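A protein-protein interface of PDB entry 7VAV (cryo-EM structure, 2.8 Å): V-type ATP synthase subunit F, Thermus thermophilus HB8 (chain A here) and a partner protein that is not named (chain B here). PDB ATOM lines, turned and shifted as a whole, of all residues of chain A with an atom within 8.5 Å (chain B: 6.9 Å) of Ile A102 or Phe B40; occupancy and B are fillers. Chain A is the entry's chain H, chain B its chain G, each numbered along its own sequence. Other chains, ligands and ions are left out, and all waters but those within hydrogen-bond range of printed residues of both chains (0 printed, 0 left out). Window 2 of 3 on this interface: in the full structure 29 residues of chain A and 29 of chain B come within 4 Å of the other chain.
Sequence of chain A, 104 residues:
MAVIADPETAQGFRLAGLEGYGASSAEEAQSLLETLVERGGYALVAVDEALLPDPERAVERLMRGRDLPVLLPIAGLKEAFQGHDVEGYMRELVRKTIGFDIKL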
ATOM      1  N   MET A  90      20.279   9.018 -25.719  1.00  0.00           N
ATOM      2  CA  MET A  90      19.821   8.572 -24.407  1.00  0.00           C
ATOM      3  C   MET A  90      18.347   8.898 -24.192  1.00  0.00           C
ATOM      4  O   MET A  90      17.607   8.098 -23.608  1.00  0.00           O
ATOM      5  CB  MET A  90      20.679   9.203 -23.312  1.00  0.00           C
ATOM      6  CG  MET A  90      22.002   8.491 -23.091  1.00  0.00           C
ATOM      7  SD  MET A  90      21.805   6.879 -22.312  1.00  0.00           S
ATOM      8  CE  MET A  90      23.307   6.066 -22.848  1.00  0.00           C
ATOM      9  N   ARG A  91      17.907  10.075 -24.645  1.00  0.00           N
ATOM     10  CA  ARG A  91      16.493  10.424 -24.541  1.00  0.00           C
ATOM     11  C   ARG A  91      15.630   9.462 -25.343  1.00  0.00           C
ATOM     12  O   ARG A  91      14.557   9.052 -24.887  1.00  0.00           O
ATOM     13  CB  ARG A  91      16.267  11.861 -25.012  1.00  0.00           C
ATOM     14  CG  ARG A  91      16.862  12.938 -24.113  1.00  0.00           C
ATOM     15  CD  ARG A  91      16.341  12.840 -22.684  1.00  0.00           C
ATOM     16  NE  ARG A  91      17.214  12.047 -21.824  1.00  0.00           N
ATOM     17  CZ  ARG A  91      18.366  12.475 -21.326  1.00  0.00           C
ATOM     18  NH1 ARG A  91      18.815  13.695 -21.571  1.00  0.00           N
ATOM     19  NH2 ARG A  91      19.083  11.660 -20.557  1.00  0.00           N
ATOM     20  N   GLU A  92      16.081   9.094 -26.544  1.00  0.00           N
ATOM     21  CA  GLU A  92      15.350   8.116 -27.342  1.00  0.00           C
ATOM     22  C   GLU A  92      15.298   6.765 -26.639  1.00  0.00           C
ATOM     23  O   GLU A  92      14.260   6.090 -26.648  1.00  0.00           O
ATOM     24  CB  GLU A  92      15.991   7.979 -28.723  1.00  0.00           C
ATOM     25  CG  GLU A  92      15.112   7.293 -29.758  1.00  0.00           C
ATOM     26  CD  GLU A  92      13.738   7.925 -29.873  1.00  0.00           C
ATOM     27  OE1 GLU A  92      13.656   9.169 -29.933  1.00  0.00           O
ATOM     28  OE2 GLU A  92      12.739   7.175 -29.909  1.00  0.00           O
ATOM     29  N   LEU A  93      16.410   6.353 -26.024  1.00  0.00           N
ATOM     30  CA  LEU A  93      16.422   5.093 -25.285  1.00  0.00           C
ATOM     31  C   LEU A  93      15.419   5.118 -24.140  1.00  0.00           C
ATOM     32  O   LEU A  93      14.664   4.159 -23.939  1.00  0.00           O
ATOM     33  CB  LEU A  93      17.825   4.805 -24.753  1.00  0.00           C
ATOM     34  CG  LEU A  93      18.893   4.376 -25.755  1.00  0.00           C
ATOM     35  CD1 LEU A  93      20.231   4.267 -25.048  1.00  0.00           C
ATOM     36  CD2 LEU A  93      18.518   3.060 -26.415  1.00  0.00           C
ATOM     37  N   VAL A  94      15.396   6.212 -23.376  1.00  0.00           N
ATOM     38  CA  VAL A  94      14.468   6.313 -22.253  1.00  0.00           C
ATOM     39  C   VAL A  94      13.027   6.331 -22.747  1.00  0.00           C
ATOM     40  O   VAL A  94      12.142   5.704 -22.148  1.00  0.00           O
ATOM     41  CB  VAL A  94      14.791   7.550 -21.395  1.00  0.00           C
ATOM     42  CG1 VAL A  94      13.800   7.675 -20.250  1.00  0.00           C
ATOM     43  CG2 VAL A  94      16.208   7.459 -20.853  1.00  0.00           C
ATOM     44  N   ARG A  95      12.764   7.051 -23.840  1.00  0.00           N
ATOM     45  CA  ARG A  95      11.414   7.100 -24.389  1.00  0.00           C
ATOM     46  C   ARG A  95      10.953   5.729 -24.863  1.00  0.00           C
ATOM     47  O   ARG A  95       9.785   5.370 -24.681  1.00  0.00           O
ATOM     48  CB  ARG A  95      11.353   8.113 -25.534  1.00  0.00           C
ATOM     49  CG  ARG A  95       9.969   8.698 -25.790  1.00  0.00           C
ATOM     50  CD  ARG A  95       9.187   7.865 -26.791  1.00  0.00           C
ATOM     51  NE  ARG A  95      10.012   7.464 -27.925  1.00  0.00           N
ATOM     52  CZ  ARG A  95       9.781   6.400 -28.680  1.00  0.00           C
ATOM     53  NH1 ARG A  95       8.751   5.601 -28.453  1.00  0.00           N
ATOM     54  NH2 ARG A  95      10.604   6.129 -29.688  1.00  0.00           N
ATOM     55  N   ILE A  98      10.408   3.505 -21.374  1.00  0.00           N
ATOM     56  CA  ILE A  98       9.306   3.810 -20.467  1.00  0.00           C
ATOM     57  C   ILE A  98       8.069   4.223 -21.252  1.00  0.00           C
ATOM     58  O   ILE A  98       6.952   3.795 -20.942  1.00  0.00           O
ATOM     59  CB  ILE A  98       9.708   4.905 -19.461  1.00  0.00           C
ATOM     60  CG1 ILE A  98      10.909   4.448 -18.632  1.00  0.00           C
ATOM     61  CG2 ILE A  98       8.539   5.253 -18.554  1.00  0.00           C
ATOM     62  CD1 ILE A  98      11.378   5.471 -17.624  1.00  0.00           C
ATOM     63  N   GLY A  99       8.257   5.050 -22.276  1.00  0.00           N
ATOM     64  CA  GLY A  99       7.155   5.569 -23.057  1.00  0.00           C
ATOM     65  C   GLY A  99       6.843   7.035 -22.848  1.00  0.00           C
ATOM     66  O   GLY A  99       5.825   7.510 -23.367  1.00  0.00           O
ATOM     67  N   PHE A 100       7.674   7.766 -22.109  1.00  0.00           N
ATOM     68  CA  PHE A 100       7.453   9.186 -21.881  1.00  0.00           C
ATOM     69  C   PHE A 100       8.794   9.906 -21.878  1.00  0.00           C
ATOM     70  O   PHE A 100       9.828   9.319 -21.549  1.00  0.00           O
ATOM     71  CB  PHE A 100       6.727   9.444 -20.555  1.00  0.00           C
ATOM     72  CG  PHE A 100       5.403   8.746 -20.440  1.00  0.00           C
ATOM     73  CD1 PHE A 100       4.258   9.311 -20.976  1.00  0.00           C
ATOM     74  CD2 PHE A 100       5.302   7.528 -19.790  1.00  0.00           C
ATOM     75  CE1 PHE A 100       3.038   8.672 -20.869  1.00  0.00           C
ATOM     76  CE2 PHE A 100       4.084   6.884 -19.679  1.00  0.00           C
ATOM     77  CZ  PHE A 100       2.952   7.457 -20.220  1.00  0.00           C
ATOM     78  N   ASP A 101       8.765  11.182 -22.253  1.00  0.00           N
ATOM     79  CA  ASP A 101       9.942  12.024 -22.101  1.00  0.00           C
ATOM     80  C   ASP A 101      10.197  12.282 -20.621  1.00  0.00           C
ATOM     81  O   ASP A 101       9.264  12.496 -19.842  1.00  0.00           O
ATOM     82  CB  ASP A 101       9.759  13.344 -22.851  1.00  0.00           C
ATOM     83  CG  ASP A 101       8.443  14.021 -22.525  1.00  0.00           C
ATOM     84  OD1 ASP A 101       7.516  13.330 -22.053  1.00  0.00           O
ATOM     85  OD2 ASP A 101       8.333  15.246 -22.747  1.00  0.00           O
ATOM     86  N   ILE A 102      11.469  12.262 -20.232  1.00  0.00           N
ATOM     87  CA  ILE A 102      11.841  12.293 -18.823  1.00  0.00           C
ATOM     88  C   ILE A 102      12.700  13.493 -18.453  1.00  0.00           C
ATOM     89  O   ILE A 102      12.835  13.787 -17.255  1.00  0.00           O
ATOM     90  CB  ILE A 102      12.550  10.987 -18.402  1.00  0.00           C
ATOM     91  CG1 ILE A 102      12.323  10.704 -16.916  1.00  0.00           C
ATOM     92  CG2 ILE A 102      14.035  11.051 -18.724  1.00  0.00           C
ATOM     93  CD1 ILE A 102      10.892  10.356 -16.575  1.00  0.00           C
ATOM     94  N   LYS A 103      13.275  14.207 -19.417  1.00  0.00           N
ATOM     95  CA  LYS A 103      14.160  15.320 -19.109  1.00  0.00           C
ATOM     96  C   LYS A 103      13.820  16.515 -19.986  1.00  0.00           C
ATOM     97  O   LYS A 103      13.283  16.368 -21.088  1.00  0.00           O
ATOM     98  CB  LYS A 103      15.635  14.938 -19.297  1.00  0.00           C
ATOM     99  CG  LYS A 103      16.169  13.990 -18.238  1.00  0.00           C
ATOM    100  CD  LYS A 103      16.094  14.610 -16.853  1.00  0.00           C
ATOM    101  CE  LYS A 103      16.995  15.828 -16.744  1.00  0.00           C
ATOM    102  NZ  LYS A 103      18.435  15.450 -16.691  1.00  0.00           N
ATOM    103  N   LEU A 104      14.140  17.702 -19.480  1.00  0.00           N
ATOM    104  CA  LEU A 104      13.926  18.944 -20.213  1.00  0.00           C
ATOM    105  C   LEU A 104      15.090  19.903 -19.987  1.00  0.00           C
ATOM    106  O   LEU A 104      15.712  19.902 -18.924  1.00  0.00           O
ATOM    107  CB  LEU A 104      12.608  19.600 -19.793  1.00  0.00           C
ATOM    108  CG  LEU A 104      12.230  20.889 -20.528  1.00  0.00           C
ATOM    109  CD1 LEU A 104      12.134  20.646 -22.027  1.00  0.00           C
ATOM    110  CD2 LEU A 104      10.929  21.464 -19.990  1.00  0.00           C
ATOM    111  OXT LEU A 104      15.439  20.703 -20.855  1.00  0.00           O
ATOM    112  N   LEU B  35      12.288  -0.630  -9.565  1.00  0.00           N
ATOM    113  CA  LEU B  35      13.010  -0.811 -10.819  1.00  0.00           C
ATOM    114  C   LEU B  35      13.236   0.520 -11.526  1.00  0.00           C
ATOM    115  O   LEU B  35      14.315   0.762 -12.075  1.00  0.00           O
ATOM    116  CB  LEU B  35      12.256  -1.784 -11.721  1.00  0.00           C
ATOM    117  CG  LEU B  35      12.444  -3.266 -11.390  1.00  0.00           C
ATOM    118  CD1 LEU B  35      11.427  -4.120 -12.128  1.00  0.00           C
ATOM    119  CD2 LEU B  35      13.861  -3.711 -11.715  1.00  0.00           C
ATOM    120  N   VAL B  36      12.230   1.398 -11.521  1.00  0.00           N
ATOM    121  CA  VAL B  36      12.390   2.722 -12.125  1.00  0.00           C
ATOM    122  C   VAL B  36      13.447   3.527 -11.375  1.00  0.00           C
ATOM    123  O   VAL B  36      14.260   4.247 -11.982  1.00  0.00           O
ATOM    124  CB  VAL B  36      11.035   3.453 -12.160  1.00  0.00           C
ATOM    125  CG1 VAL B  36      11.225   4.935 -12.444  1.00  0.00           C
ATOM    126  CG2 VAL B  36      10.121   2.819 -13.197  1.00  0.00           C
ATOM    127  N   ALA B  37      13.445   3.427 -10.041  1.00  0.00           N
ATOM    128  CA  ALA B  37      14.443   4.134  -9.246  1.00  0.00           C
ATOM    129  C   ALA B  37      15.853   3.695  -9.619  1.00  0.00           C
ATOM    130  O   ALA B  37      16.762   4.527  -9.724  1.00  0.00           O
ATOM    131  CB  ALA B  37      14.183   3.908  -7.758  1.00  0.00           C
ATOM    132  N   GLU B  38      16.057   2.393  -9.819  1.00  0.00           N
ATOM    133  CA  GLU B  38      17.365   1.923 -10.277  1.00  0.00           C
ATOM    134  C   GLU B  38      17.653   2.379 -11.707  1.00  0.00           C
ATOM    135  O   GLU B  38      18.801   2.709 -12.048  1.00  0.00           O
ATOM    136  CB  GLU B  38      17.446   0.402 -10.172  1.00  0.00           C
ATOM    137  CG  GLU B  38      18.762  -0.178 -10.661  1.00  0.00           C
ATOM    138  CD  GLU B  38      19.001  -1.589 -10.167  1.00  0.00           C
ATOM    139  OE1 GLU B  38      18.065  -2.182  -9.593  1.00  0.00           O
ATOM    140  OE2 GLU B  38      20.124  -2.103 -10.350  1.00  0.00           O
ATOM    141  N   PHE B  39      16.620   2.399 -12.552  1.00  0.00           N
ATOM    142  CA  PHE B  39      16.793   2.747 -13.958  1.00  0.00           C
ATOM    143  C   PHE B  39      17.317   4.164 -14.120  1.00  0.00           C
ATOM    144  O   PHE B  39      18.123   4.436 -15.017  1.00  0.00           O
ATOM    145  CB  PHE B  39      15.464   2.580 -14.695  1.00  0.00           C
ATOM    146  CG  PHE B  39      15.500   3.020 -16.130  1.00  0.00           C
ATOM    147  CD1 PHE B  39      16.088   2.223 -17.097  1.00  0.00           C
ATOM    148  CD2 PHE B  39      14.930   4.221 -16.514  1.00  0.00           C
ATOM    149  CE1 PHE B  39      16.116   2.622 -18.419  1.00  0.00           C
ATOM    150  CE2 PHE B  39      14.953   4.624 -17.834  1.00  0.00           C
ATOM    151  CZ  PHE B  39      15.547   3.823 -18.787  1.00  0.00           C
ATOM    152  N   PHE B  40      16.853   5.089 -13.277  1.00  0.00           N
ATOM    153  CA  PHE B  40      17.323   6.470 -13.392  1.00  0.00           C
ATOM    154  C   PHE B  40      18.830   6.574 -13.146  1.00  0.00           C
ATOM    155  O   PHE B  40      19.551   7.248 -13.900  1.00  0.00           O
ATOM    156  CB  PHE B  40      16.552   7.370 -12.430  1.00  0.00           C
ATOM    157  CG  PHE B  40      15.188   7.752 -12.927  1.00  0.00           C
ATOM    158  CD1 PHE B  40      14.899   7.725 -14.281  1.00  0.00           C
ATOM    159  CD2 PHE B  40      14.194   8.140 -12.043  1.00  0.00           C
ATOM    160  CE1 PHE B  40      13.646   8.075 -14.746  1.00  0.00           C
ATOM    161  CE2 PHE B  40      12.937   8.491 -12.502  1.00  0.00           C
ATOM    162  CZ  PHE B  40      12.664   8.459 -13.856  1.00  0.00           C
ATOM    163  N   GLY B  41      19.327   5.905 -12.103  1.00  0.00           N
ATOM    164  CA  GLY B  41      20.757   5.918 -11.844  1.00  0.00           C
ATOM    165  C   GLY B  41      21.553   5.236 -12.940  1.00  0.00           C
ATOM    166  O   GLY B  41      22.646   5.688 -13.305  1.00  0.00           O
ATOM    167  N   LEU B  42      21.019   4.136 -13.479  1.00  0.00           N
ATOM    168  CA  LEU B  42      21.676   3.494 -14.614  1.00  0.00           C
ATOM    169  C   LEU B  42      21.758   4.437 -15.809  1.00  0.00           C
ATOM    170  O   LEU B  42      22.779   4.474 -16.507  1.00  0.00           O
ATOM    171  CB  LEU B  42      20.955   2.201 -14.992  1.00  0.00           C
ATOM    172  CG  LEU B  42      21.449   0.918 -14.319  1.00  0.00           C
ATOM    173  CD1 LEU B  42      22.875   0.642 -14.753  1.00  0.00           C
ATOM    174  CD2 LEU B  42      21.374   1.000 -12.808  1.00  0.00           C
ATOM    175  N   VAL B  43      20.699   5.208 -16.058  1.00  0.00           N
ATOM    176  CA  VAL B  43      20.710   6.169 -17.160  1.00  0.00           C
ATOM    177  C   VAL B  43      21.790   7.221 -16.936  1.00  0.00           C
ATOM    178  O   VAL B  43      22.532   7.586 -17.858  1.00  0.00           O
ATOM    179  CB  VAL B  43      19.322   6.814 -17.324  1.00  0.00           C
ATOM    180  CG1 VAL B  43      19.416   8.089 -18.149  1.00  0.00           C
ATOM    181  CG2 VAL B  43      18.358   5.835 -17.966  1.00  0.00           C
ATOM    182  N   ARG B  44      21.888   7.732 -15.705  1.00  0.00           N
ATOM    183  CA  ARG B  44      22.906   8.741 -15.410  1.00  0.00           C
ATOM    184  C   ARG B  44      24.313   8.195 -15.646  1.00  0.00           C
ATOM    185  O   ARG B  44      25.150   8.844 -16.296  1.00  0.00           O
ATOM    186  CB  ARG B  44      22.758   9.234 -13.971  1.00  0.00           C
ATOM    187  CG  ARG B  44      21.776  10.380 -13.801  1.00  0.00           C
ATOM    188  CD  ARG B  44      21.774  10.892 -12.369  1.00  0.00           C
ATOM    189  NE  ARG B  44      21.150   9.948 -11.451  1.00  0.00           N
ATOM    190  CZ  ARG B  44      19.850   9.899 -11.194  1.00  0.00           C
ATOM    191  NH1 ARG B  44      19.000  10.732 -11.771  1.00  0.00           N
ATOM    192  NH2 ARG B  44      19.391   8.992 -10.336  1.00  0.00           N
ATOM    193  N   GLU B  45      24.592   6.995 -15.128  1.00  0.00           N
ATOM    194  CA  GLU B  45      25.929   6.439 -15.300  1.00  0.00           C
ATOM    195  C   GLU B  45      26.210   6.100 -16.761  1.00  0.00           C
ATOM    196  O   GLU B  45      27.356   6.218 -17.212  1.00  0.00           O
ATOM    197  CB  GLU B  45      26.123   5.211 -14.406  1.00  0.00           C
ATOM    198  CG  GLU B  45      25.715   3.884 -15.019  1.00  0.00           C
ATOM    199  CD  GLU B  45      26.124   2.705 -14.161  1.00  0.00           C
ATOM    200  OE1 GLU B  45      26.592   2.929 -13.025  1.00  0.00           O
ATOM    201  OE2 GLU B  45      25.988   1.554 -14.624  1.00  0.00           O
ATOM    202  N   ALA B  46      25.183   5.704 -17.519  1.00  0.00           N
ATOM    203  CA  ALA B  46      25.373   5.448 -18.942  1.00  0.00           C
ATOM    204  C   ALA B  46      25.707   6.730 -19.690  1.00  0.00           C
ATOM    205  O   ALA B  46      26.551   6.726 -20.591  1.00  0.00           O
ATOM    206  CB  ALA B  46      24.127   4.789 -19.529  1.00  0.00           C
ATOM    207  N   ILE B 150      17.396  -3.692 -17.287  1.00  0.00           N
ATOM    208  CA  ILE B 150      16.482  -2.995 -16.387  1.00  0.00           C
ATOM    209  C   ILE B 150      15.218  -2.579 -17.127  1.00  0.00           C
ATOM    210  O   ILE B 150      14.102  -2.713 -16.609  1.00  0.00           O
ATOM    211  CB  ILE B 150      17.185  -1.786 -15.742  1.00  0.00           C
ATOM    212  CG1 ILE B 150      18.275  -2.259 -14.779  1.00  0.00           C
ATOM    213  CG2 ILE B 150      16.182  -0.913 -15.015  1.00  0.00           C
ATOM    214  CD1 ILE B 150      17.736  -2.872 -13.507  1.00  0.00           C
ATOM    215  N   ILE B 154      11.352  -3.658 -16.386  1.00  0.00           N
ATOM    216  CA  ILE B 154      10.312  -2.654 -16.169  1.00  0.00           C
ATOM    217  C   ILE B 154       9.132  -2.898 -17.101  1.00  0.00           C
ATOM    218  O   ILE B 154       7.967  -2.825 -16.685  1.00  0.00           O
ATOM    219  CB  ILE B 154      10.892  -1.239 -16.350  1.00  0.00           C
ATOM    220  CG1 ILE B 154      11.697  -0.829 -15.118  1.00  0.00           C
ATOM    221  CG2 ILE B 154       9.785  -0.232 -16.617  1.00  0.00           C
ATOM    222  CD1 ILE B 154      12.343   0.530 -15.238  1.00  0.00           C
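Among the printed residues, pairs that only touch across the chains: Met A90 with Ala B46, Ile A102 with Phe B40, Ile A98 with Phe B39 and Val A94 with Val B43.
Of the printed residues of chain B, Met A90 touches Ala B46. Of the printed residues of chain B, Val A94 touches Val B43. Of the printed residues of chain B, Ile A98 touches Phe B39. Ile A102 touches just one residue of chain B: Phe B40. Printed residues of chain A within 4 Å of Phe B39: Ile A98. Of the printed residues of chain A, Phe B40 touches Ile A102. Of the printed residues of chain A, Ala B46 touches Met A90 (3.6 Å). The nearest residue of chain B that does not touch Ile A102 is Val B43 (6.2 Å). The nearest residue of chain A that does not touch Phe B40 is Ile A98 (4.5 Å). The nearest printed residue of chain A that does not touch Val B43 is Arg A91 (4.3 Å).
Of the 13 printed residues of chain A, 4 touch a printed residue of chain B. Hydrophobic or aromatic side chains of chain A that line the printed part of chain B: Met A90, Val A94, Ile A98 and Ile A102. Of the 14 printed residues of chain B, 4 touch a printed residue of chain A. Hydrophobic or aromatic side chains of chain B that line the printed part of chain A: Phe B39, Phe B40, Val B43 and Ala B46. Among the printed residues, 4 pairs touch across the chains. Among the printed residues, no Asp or Glu carboxylate lies within 4 Å of a Lys or Arg side-chain nitrogen of the other chain.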
